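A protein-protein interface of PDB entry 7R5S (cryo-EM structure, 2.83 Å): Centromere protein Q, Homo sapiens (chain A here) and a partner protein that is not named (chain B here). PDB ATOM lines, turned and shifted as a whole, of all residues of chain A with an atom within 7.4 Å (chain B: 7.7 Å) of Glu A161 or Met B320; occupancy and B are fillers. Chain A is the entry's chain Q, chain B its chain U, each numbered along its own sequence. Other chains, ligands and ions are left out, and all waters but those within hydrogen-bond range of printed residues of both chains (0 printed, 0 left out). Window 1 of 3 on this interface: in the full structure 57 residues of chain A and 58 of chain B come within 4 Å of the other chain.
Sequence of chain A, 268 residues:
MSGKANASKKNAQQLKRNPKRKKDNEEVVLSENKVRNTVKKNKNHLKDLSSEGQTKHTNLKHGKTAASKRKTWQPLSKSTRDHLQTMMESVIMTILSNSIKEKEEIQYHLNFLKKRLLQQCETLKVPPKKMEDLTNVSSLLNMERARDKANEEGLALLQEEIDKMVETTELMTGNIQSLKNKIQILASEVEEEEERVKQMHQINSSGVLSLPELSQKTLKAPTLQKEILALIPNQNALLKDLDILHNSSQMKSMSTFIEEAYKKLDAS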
ATOM      1  N   GLY A 154      28.477  33.681  21.123  1.00  0.00           N
ATOM      2  CA  GLY A 154      28.088  32.589  20.245  1.00  0.00           C
ATOM      3  C   GLY A 154      26.800  31.919  20.684  1.00  0.00           C
ATOM      4  O   GLY A 154      25.920  31.643  19.863  1.00  0.00           O
ATOM      5  N   LEU A 155      26.673  31.650  21.987  1.00  0.00           N
ATOM      6  CA  LEU A 155      25.449  31.048  22.502  1.00  0.00           C
ATOM      7  C   LEU A 155      24.254  31.966  22.292  1.00  0.00           C
ATOM      8  O   LEU A 155      23.155  31.500  21.973  1.00  0.00           O
ATOM      9  CB  LEU A 155      25.616  30.709  23.983  1.00  0.00           C
ATOM     10  CG  LEU A 155      24.440  30.008  24.667  1.00  0.00           C
ATOM     11  CD1 LEU A 155      24.085  28.723  23.939  1.00  0.00           C
ATOM     12  CD2 LEU A 155      24.763  29.728  26.126  1.00  0.00           C
ATOM     13  N   ALA A 156      24.451  33.277  22.454  1.00  0.00           N
ATOM     14  CA  ALA A 156      23.360  34.220  22.226  1.00  0.00           C
ATOM     15  C   ALA A 156      22.896  34.183  20.775  1.00  0.00           C
ATOM     16  O   ALA A 156      21.690  34.148  20.495  1.00  0.00           O
ATOM     17  CB  ALA A 156      23.796  35.631  22.620  1.00  0.00           C
ATOM     18  N   LEU A 157      23.845  34.192  19.835  1.00  0.00           N
ATOM     19  CA  LEU A 157      23.482  34.127  18.421  1.00  0.00           C
ATOM     20  C   LEU A 157      22.737  32.833  18.101  1.00  0.00           C
ATOM     21  O   LEU A 157      21.699  32.847  17.422  1.00  0.00           O
ATOM     22  CB  LEU A 157      24.732  34.259  17.551  1.00  0.00           C
ATOM     23  CG  LEU A 157      25.464  35.602  17.610  1.00  0.00           C
ATOM     24  CD1 LEU A 157      26.722  35.567  16.757  1.00  0.00           C
ATOM     25  CD2 LEU A 157      24.545  36.730  17.170  1.00  0.00           C
ATOM     26  N   LEU A 158      23.261  31.701  18.582  1.00  0.00           N
ATOM     27  CA  LEU A 158      22.610  30.420  18.322  1.00  0.00           C
ATOM     28  C   LEU A 158      21.203  30.387  18.904  1.00  0.00           C
ATOM     29  O   LEU A 158      20.269  29.888  18.264  1.00  0.00           O
ATOM     30  CB  LEU A 158      23.450  29.273  18.886  1.00  0.00           C
ATOM     31  CG  LEU A 158      24.855  29.077  18.308  1.00  0.00           C
ATOM     32  CD1 LEU A 158      25.529  27.866  18.935  1.00  0.00           C
ATOM     33  CD2 LEU A 158      24.814  28.947  16.795  1.00  0.00           C
ATOM     34  N   GLN A 159      21.027  30.927  20.113  1.00  0.00           N
ATOM     35  CA  GLN A 159      19.710  30.922  20.738  1.00  0.00           C
ATOM     36  C   GLN A 159      18.731  31.801  19.972  1.00  0.00           C
ATOM     37  O   GLN A 159      17.563  31.435  19.807  1.00  0.00           O
ATOM     38  CB  GLN A 159      19.818  31.379  22.193  1.00  0.00           C
ATOM     39  CG  GLN A 159      18.555  31.155  23.007  1.00  0.00           C
ATOM     40  CD  GLN A 159      18.204  29.686  23.143  1.00  0.00           C
ATOM     41  OE1 GLN A 159      19.085  28.833  23.248  1.00  0.00           O
ATOM     42  NE2 GLN A 159      16.911  29.384  23.142  1.00  0.00           N
ATOM     43  N   GLU A 160      19.187  32.962  19.493  1.00  0.00           N
ATOM     44  CA  GLU A 160      18.309  33.828  18.709  1.00  0.00           C
ATOM     45  C   GLU A 160      17.865  33.136  17.425  1.00  0.00           C
ATOM     46  O   GLU A 160      16.683  33.188  17.047  1.00  0.00           O
ATOM     47  CB  GLU A 160      19.020  35.146  18.400  1.00  0.00           C
ATOM     48  CG  GLU A 160      18.132  36.371  18.513  1.00  0.00           C
ATOM     49  CD  GLU A 160      17.173  36.499  17.348  1.00  0.00           C
ATOM     50  OE1 GLU A 160      17.540  36.085  16.229  1.00  0.00           O
ATOM     51  OE2 GLU A 160      16.053  37.010  17.551  1.00  0.00           O
ATOM     52  N   GLU A 161      18.805  32.476  16.740  1.00  0.00           N
ATOM     53  CA  GLU A 161      18.447  31.738  15.532  1.00  0.00           C
ATOM     54  C   GLU A 161      17.450  30.626  15.838  1.00  0.00           C
ATOM     55  O   GLU A 161      16.487  30.417  15.087  1.00  0.00           O
ATOM     56  CB  GLU A 161      19.703  31.170  14.872  1.00  0.00           C
ATOM     57  CG  GLU A 161      20.702  32.222  14.413  1.00  0.00           C
ATOM     58  CD  GLU A 161      20.207  33.028  13.228  1.00  0.00           C
ATOM     59  OE1 GLU A 161      19.315  32.540  12.502  1.00  0.00           O
ATOM     60  OE2 GLU A 161      20.711  34.151  13.020  1.00  0.00           O
ATOM     61  N   ILE A 162      17.660  29.904  16.943  1.00  0.00           N
ATOM     62  CA  ILE A 162      16.750  28.822  17.309  1.00  0.00           C
ATOM     63  C   ILE A 162      15.355  29.368  17.591  1.00  0.00           C
ATOM     64  O   ILE A 162      14.348  28.780  17.175  1.00  0.00           O
ATOM     65  CB  ILE A 162      17.306  28.036  18.510  1.00  0.00           C
ATOM     66  CG1 ILE A 162      18.532  27.222  18.090  1.00  0.00           C
ATOM     67  CG2 ILE A 162      16.241  27.126  19.101  1.00  0.00           C
ATOM     68  CD1 ILE A 162      19.150  26.425  19.217  1.00  0.00           C
ATOM     69  N   ASP A 163      15.271  30.500  18.295  1.00  0.00           N
ATOM     70  CA  ASP A 163      13.967  31.086  18.595  1.00  0.00           C
ATOM     71  C   ASP A 163      13.235  31.494  17.322  1.00  0.00           C
ATOM     72  O   ASP A 163      12.041  31.209  17.162  1.00  0.00           O
ATOM     73  CB  ASP A 163      14.118  32.283  19.536  1.00  0.00           C
ATOM     74  CG  ASP A 163      14.877  31.941  20.801  1.00  0.00           C
ATOM     75  OD1 ASP A 163      15.583  32.824  21.331  1.00  0.00           O
ATOM     76  OD2 ASP A 163      14.763  30.788  21.270  1.00  0.00           O
ATOM     77  N   LYS A 164      13.932  32.174  16.404  1.00  0.00           N
ATOM     78  CA  LYS A 164      13.256  32.591  15.178  1.00  0.00           C
ATOM     79  C   LYS A 164      12.817  31.390  14.346  1.00  0.00           C
ATOM     80  O   LYS A 164      11.711  31.392  13.783  1.00  0.00           O
ATOM     81  CB  LYS A 164      14.146  33.536  14.361  1.00  0.00           C
ATOM     82  CG  LYS A 164      15.293  32.883  13.609  1.00  0.00           C
ATOM     83  CD  LYS A 164      15.933  33.851  12.627  1.00  0.00           C
ATOM     84  CE  LYS A 164      16.462  35.088  13.332  1.00  0.00           C
ATOM     85  NZ  LYS A 164      16.835  36.160  12.369  1.00  0.00           N
ATOM     86  N   MET A 165      13.639  30.336  14.292  1.00  0.00           N
ATOM     87  CA  MET A 165      13.256  29.143  13.545  1.00  0.00           C
ATOM     88  C   MET A 165      12.050  28.460  14.178  1.00  0.00           C
ATOM     89  O   MET A 165      11.158  27.973  13.472  1.00  0.00           O
ATOM     90  CB  MET A 165      14.438  28.179  13.455  1.00  0.00           C
ATOM     91  CG  MET A 165      15.482  28.569  12.424  1.00  0.00           C
ATOM     92  SD  MET A 165      16.788  27.337  12.270  1.00  0.00           S
ATOM     93  CE  MET A 165      17.701  27.989  10.876  1.00  0.00           C
ATOM     94  N   VAL A 166      12.004  28.418  15.513  1.00  0.00           N
ATOM     95  CA  VAL A 166      10.881  27.787  16.202  1.00  0.00           C
ATOM     96  C   VAL A 166       9.594  28.560  15.941  1.00  0.00           C
ATOM     97  O   VAL A 166       8.538  27.967  15.679  1.00  0.00           O
ATOM     98  CB  VAL A 166      11.180  27.666  17.708  1.00  0.00           C
ATOM     99  CG1 VAL A 166       9.896  27.458  18.497  1.00  0.00           C
ATOM    100  CG2 VAL A 166      12.151  26.524  17.962  1.00  0.00           C
ATOM    101  N   GLU A 167       9.658  29.892  16.009  1.00  0.00           N
ATOM    102  CA  GLU A 167       8.488  30.706  15.688  1.00  0.00           C
ATOM    103  C   GLU A 167       8.007  30.428  14.268  1.00  0.00           C
ATOM    104  O   GLU A 167       6.807  30.220  14.026  1.00  0.00           O
ATOM    105  CB  GLU A 167       8.812  32.190  15.871  1.00  0.00           C
ATOM    106  CG  GLU A 167       9.210  32.573  17.287  1.00  0.00           C
ATOM    107  CD  GLU A 167       9.870  33.937  17.356  1.00  0.00           C
ATOM    108  OE1 GLU A 167       9.855  34.658  16.337  1.00  0.00           O
ATOM    109  OE2 GLU A 167      10.405  34.286  18.429  1.00  0.00           O
ATOM    110  N   LYS B 315      25.614  21.407  22.415  1.00  0.00           N
ATOM    111  CA  LYS B 315      24.290  20.796  22.487  1.00  0.00           C
ATOM    112  C   LYS B 315      23.273  21.565  21.646  1.00  0.00           C
ATOM    113  O   LYS B 315      22.414  20.959  20.996  1.00  0.00           O
ATOM    114  CB  LYS B 315      23.830  20.713  23.942  1.00  0.00           C
ATOM    115  CG  LYS B 315      22.505  19.997  24.136  1.00  0.00           C
ATOM    116  CD  LYS B 315      22.095  19.986  25.600  1.00  0.00           C
ATOM    117  CE  LYS B 315      21.933  21.399  26.138  1.00  0.00           C
ATOM    118  NZ  LYS B 315      21.518  21.406  27.568  1.00  0.00           N
ATOM    119  N   LYS B 316      23.355  22.898  21.647  1.00  0.00           N
ATOM    120  CA  LYS B 316      22.365  23.707  20.935  1.00  0.00           C
ATOM    121  C   LYS B 316      22.516  23.605  19.421  1.00  0.00           C
ATOM    122  O   LYS B 316      21.540  23.824  18.682  1.00  0.00           O
ATOM    123  CB  LYS B 316      22.468  25.168  21.374  1.00  0.00           C
ATOM    124  CG  LYS B 316      21.986  25.432  22.790  1.00  0.00           C
ATOM    125  CD  LYS B 316      20.474  25.323  22.890  1.00  0.00           C
ATOM    126  CE  LYS B 316      19.980  25.749  24.262  1.00  0.00           C
ATOM    127  NZ  LYS B 316      18.495  25.715  24.354  1.00  0.00           N
ATOM    128  N   ARG B 317      23.727  23.311  18.939  1.00  0.00           N
ATOM    129  CA  ARG B 317      23.936  23.191  17.496  1.00  0.00           C
ATOM    130  C   ARG B 317      23.019  22.135  16.877  1.00  0.00           C
ATOM    131  O   ARG B 317      22.409  22.368  15.821  1.00  0.00           O
ATOM    132  CB  ARG B 317      25.401  22.862  17.209  1.00  0.00           C
ATOM    133  CG  ARG B 317      25.821  23.074  15.767  1.00  0.00           C
ATOM    134  CD  ARG B 317      27.305  22.800  15.590  1.00  0.00           C
ATOM    135  NE  ARG B 317      28.116  23.575  16.524  1.00  0.00           N
ATOM    136  CZ  ARG B 317      29.425  23.411  16.692  1.00  0.00           C
ATOM    137  NH1 ARG B 317      30.075  22.494  15.988  1.00  0.00           N
ATOM    138  NH2 ARG B 317      30.082  24.161  17.565  1.00  0.00           N
ATOM    139  N   GLN B 318      22.906  20.970  17.519  1.00  0.00           N
ATOM    140  CA  GLN B 318      22.078  19.897  16.973  1.00  0.00           C
ATOM    141  C   GLN B 318      20.602  20.277  16.980  1.00  0.00           C
ATOM    142  O   GLN B 318      19.857  19.913  16.062  1.00  0.00           O
ATOM    143  CB  GLN B 318      22.303  18.608  17.763  1.00  0.00           C
ATOM    144  CG  GLN B 318      23.740  18.117  17.751  1.00  0.00           C
ATOM    145  CD  GLN B 318      23.918  16.827  18.528  1.00  0.00           C
ATOM    146  OE1 GLN B 318      22.948  16.231  18.995  1.00  0.00           O
ATOM    147  NE2 GLN B 318      25.163  16.388  18.669  1.00  0.00           N
ATOM    148  N   ARG B 319      20.160  20.997  18.014  1.00  0.00           N
ATOM    149  CA  ARG B 319      18.784  21.484  18.041  1.00  0.00           C
ATOM    150  C   ARG B 319      18.514  22.417  16.869  1.00  0.00           C
ATOM    151  O   ARG B 319      17.470  22.316  16.209  1.00  0.00           O
ATOM    152  CB  ARG B 319      18.508  22.191  19.368  1.00  0.00           C
ATOM    153  CG  ARG B 319      17.185  22.932  19.418  1.00  0.00           C
ATOM    154  CD  ARG B 319      16.011  21.970  19.472  1.00  0.00           C
ATOM    155  NE  ARG B 319      14.732  22.673  19.489  1.00  0.00           N
ATOM    156  CZ  ARG B 319      14.166  23.165  20.587  1.00  0.00           C
ATOM    157  NH1 ARG B 319      14.765  23.032  21.762  1.00  0.00           N
ATOM    158  NH2 ARG B 319      12.999  23.791  20.509  1.00  0.00           N
ATOM    159  N   MET B 320      19.444  23.335  16.597  1.00  0.00           N
ATOM    160  CA  MET B 320      19.293  24.211  15.436  1.00  0.00           C
ATOM    161  C   MET B 320      19.180  23.401  14.148  1.00  0.00           C
ATOM    162  O   MET B 320      18.306  23.659  13.306  1.00  0.00           O
ATOM    163  CB  MET B 320      20.469  25.184  15.354  1.00  0.00           C
ATOM    164  CG  MET B 320      20.586  25.893  14.016  1.00  0.00           C
ATOM    165  SD  MET B 320      22.028  26.966  13.914  1.00  0.00           S
ATOM    166  CE  MET B 320      21.655  28.137  15.214  1.00  0.00           C
ATOM    167  N   ILE B 321      20.061  22.410  13.985  1.00  0.00           N
ATOM    168  CA  ILE B 321      20.058  21.601  12.767  1.00  0.00           C
ATOM    169  C   ILE B 321      18.725  20.878  12.599  1.00  0.00           C
ATOM    170  O   ILE B 321      18.141  20.859  11.505  1.00  0.00           O
ATOM    171  CB  ILE B 321      21.241  20.614  12.779  1.00  0.00           C
ATOM    172  CG1 ILE B 321      22.566  21.370  12.674  1.00  0.00           C
ATOM    173  CG2 ILE B 321      21.108  19.603  11.650  1.00  0.00           C
ATOM    174  CD1 ILE B 321      23.780  20.469  12.617  1.00  0.00           C
ATOM    175  N   GLU B 322      18.215  20.278  13.679  1.00  0.00           N
ATOM    176  CA  GLU B 322      16.979  19.508  13.560  1.00  0.00           C
ATOM    177  C   GLU B 322      15.771  20.408  13.326  1.00  0.00           C
ATOM    178  O   GLU B 322      14.844  20.018  12.606  1.00  0.00           O
ATOM    179  CB  GLU B 322      16.776  18.628  14.796  1.00  0.00           C
ATOM    180  CG  GLU B 322      16.450  19.370  16.078  1.00  0.00           C
ATOM    181  CD  GLU B 322      16.373  18.448  17.279  1.00  0.00           C
ATOM    182  OE1 GLU B 322      16.864  17.304  17.184  1.00  0.00           O
ATOM    183  OE2 GLU B 322      15.822  18.868  18.319  1.00  0.00           O
ATOM    184  N   VAL B 323      15.766  21.621  13.889  1.00  0.00           N
ATOM    185  CA  VAL B 323      14.657  22.528  13.608  1.00  0.00           C
ATOM    186  C   VAL B 323      14.689  22.980  12.150  1.00  0.00           C
ATOM    187  O   VAL B 323      13.636  23.091  11.499  1.00  0.00           O
ATOM    188  CB  VAL B 323      14.680  23.725  14.576  1.00  0.00           C
ATOM    189  CG1 VAL B 323      13.637  24.753  14.177  1.00  0.00           C
ATOM    190  CG2 VAL B 323      14.435  23.256  16.000  1.00  0.00           C
ATOM    191  N   GLN B 324      15.885  23.233  11.609  1.00  0.00           N
ATOM    192  CA  GLN B 324      15.987  23.559  10.188  1.00  0.00           C
ATOM    193  C   GLN B 324      15.472  22.413   9.324  1.00  0.00           C
ATOM    194  O   GLN B 324      14.742  22.637   8.347  1.00  0.00           O
ATOM    195  CB  GLN B 324      17.433  23.900   9.828  1.00  0.00           C
ATOM    196  CG  GLN B 324      17.672  24.108   8.341  1.00  0.00           C
ATOM    197  CD  GLN B 324      16.792  25.190   7.751  1.00  0.00           C
ATOM    198  OE1 GLN B 324      16.972  26.375   8.030  1.00  0.00           O
ATOM    199  NE2 GLN B 324      15.830  24.787   6.929  1.00  0.00           N
ATOM    200  N   ASP B 325      15.847  21.176   9.670  1.00  0.00           N
ATOM    201  CA  ASP B 325      15.339  20.015   8.942  1.00  0.00           C
ATOM    202  C   ASP B 325      13.817  19.949   8.995  1.00  0.00           C
ATOM    203  O   ASP B 325      13.162  19.672   7.981  1.00  0.00           O
ATOM    204  CB  ASP B 325      15.943  18.731   9.510  1.00  0.00           C
ATOM    205  CG  ASP B 325      17.265  18.371   8.865  1.00  0.00           C
ATOM    206  OD1 ASP B 325      18.305  18.915   9.291  1.00  0.00           O
ATOM    207  OD2 ASP B 325      17.266  17.542   7.931  1.00  0.00           O
ATOM    208  N   GLU B 326      13.239  20.201  10.172  1.00  0.00           N
ATOM    209  CA  GLU B 326      11.787  20.151  10.317  1.00  0.00           C
ATOM    210  C   GLU B 326      11.106  21.176   9.418  1.00  0.00           C
ATOM    211  O   GLU B 326      10.129  20.864   8.727  1.00  0.00           O
ATOM    212  CB  GLU B 326      11.401  20.374  11.779  1.00  0.00           C
ATOM    213  CG  GLU B 326       9.902  20.386  12.039  1.00  0.00           C
ATOM    214  CD  GLU B 326       9.295  18.995  12.058  1.00  0.00           C
ATOM    215  OE1 GLU B 326      10.053  18.007  11.956  1.00  0.00           O
ATOM    216  OE2 GLU B 326       8.056  18.889  12.181  1.00  0.00           O
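OD2 of Asp A163 lies within hydrogen-bond range of NE2 of Gln A159 (3.2 Å).
Among the printed residues, pairs that only touch across the chains: Met A165 with Gln B324, Ile A162 with Lys B316, Met A165 with Val B323, Glu A161 with Met B320, Leu A158 with Met B320, Val A166 with Arg B319 and Ile A162 with Met B320.
The side-chain amide oxygen of Gln A159 is in hydrogen-bond range of the side-chain amino group of Lys B316, 3.4 Å away.
Of the 12 printed residues of chain B, 5 touch a printed residue of chain A. Hydrophobic or aromatic side chains of chain A within 4 Å of the printed part of chain B: Leu A158, Ile A162, Met A165 and Val A166. Along chain A the printed residues that touch a printed residue of chain B span positions 158 to 166.
Of the printed residues of chain B, Leu A158 touches Met B320 (3.6 Å). Glu A161 touches just one residue of chain B: Met B320. Of the printed residues of chain B, Ile A162 touches Lys B316 and Met B320. Of the printed residues of chain B, Met A165 touches Val B323 and Gln B324. Of the printed residues of chain B, Val A166 touches Arg B319 (3.8 Å). Met B320 touches just these residues of chain A: Leu A158 (3.6 Å), Glu A161 (3.6 Å) and Ile A162 (3.9 Å). Of the printed residues of chain A, Gln B324 touches Met A165 (3.4 Å). The nearest residue of chain B that does not touch Glu A161 is Val B323 (6.4 Å).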
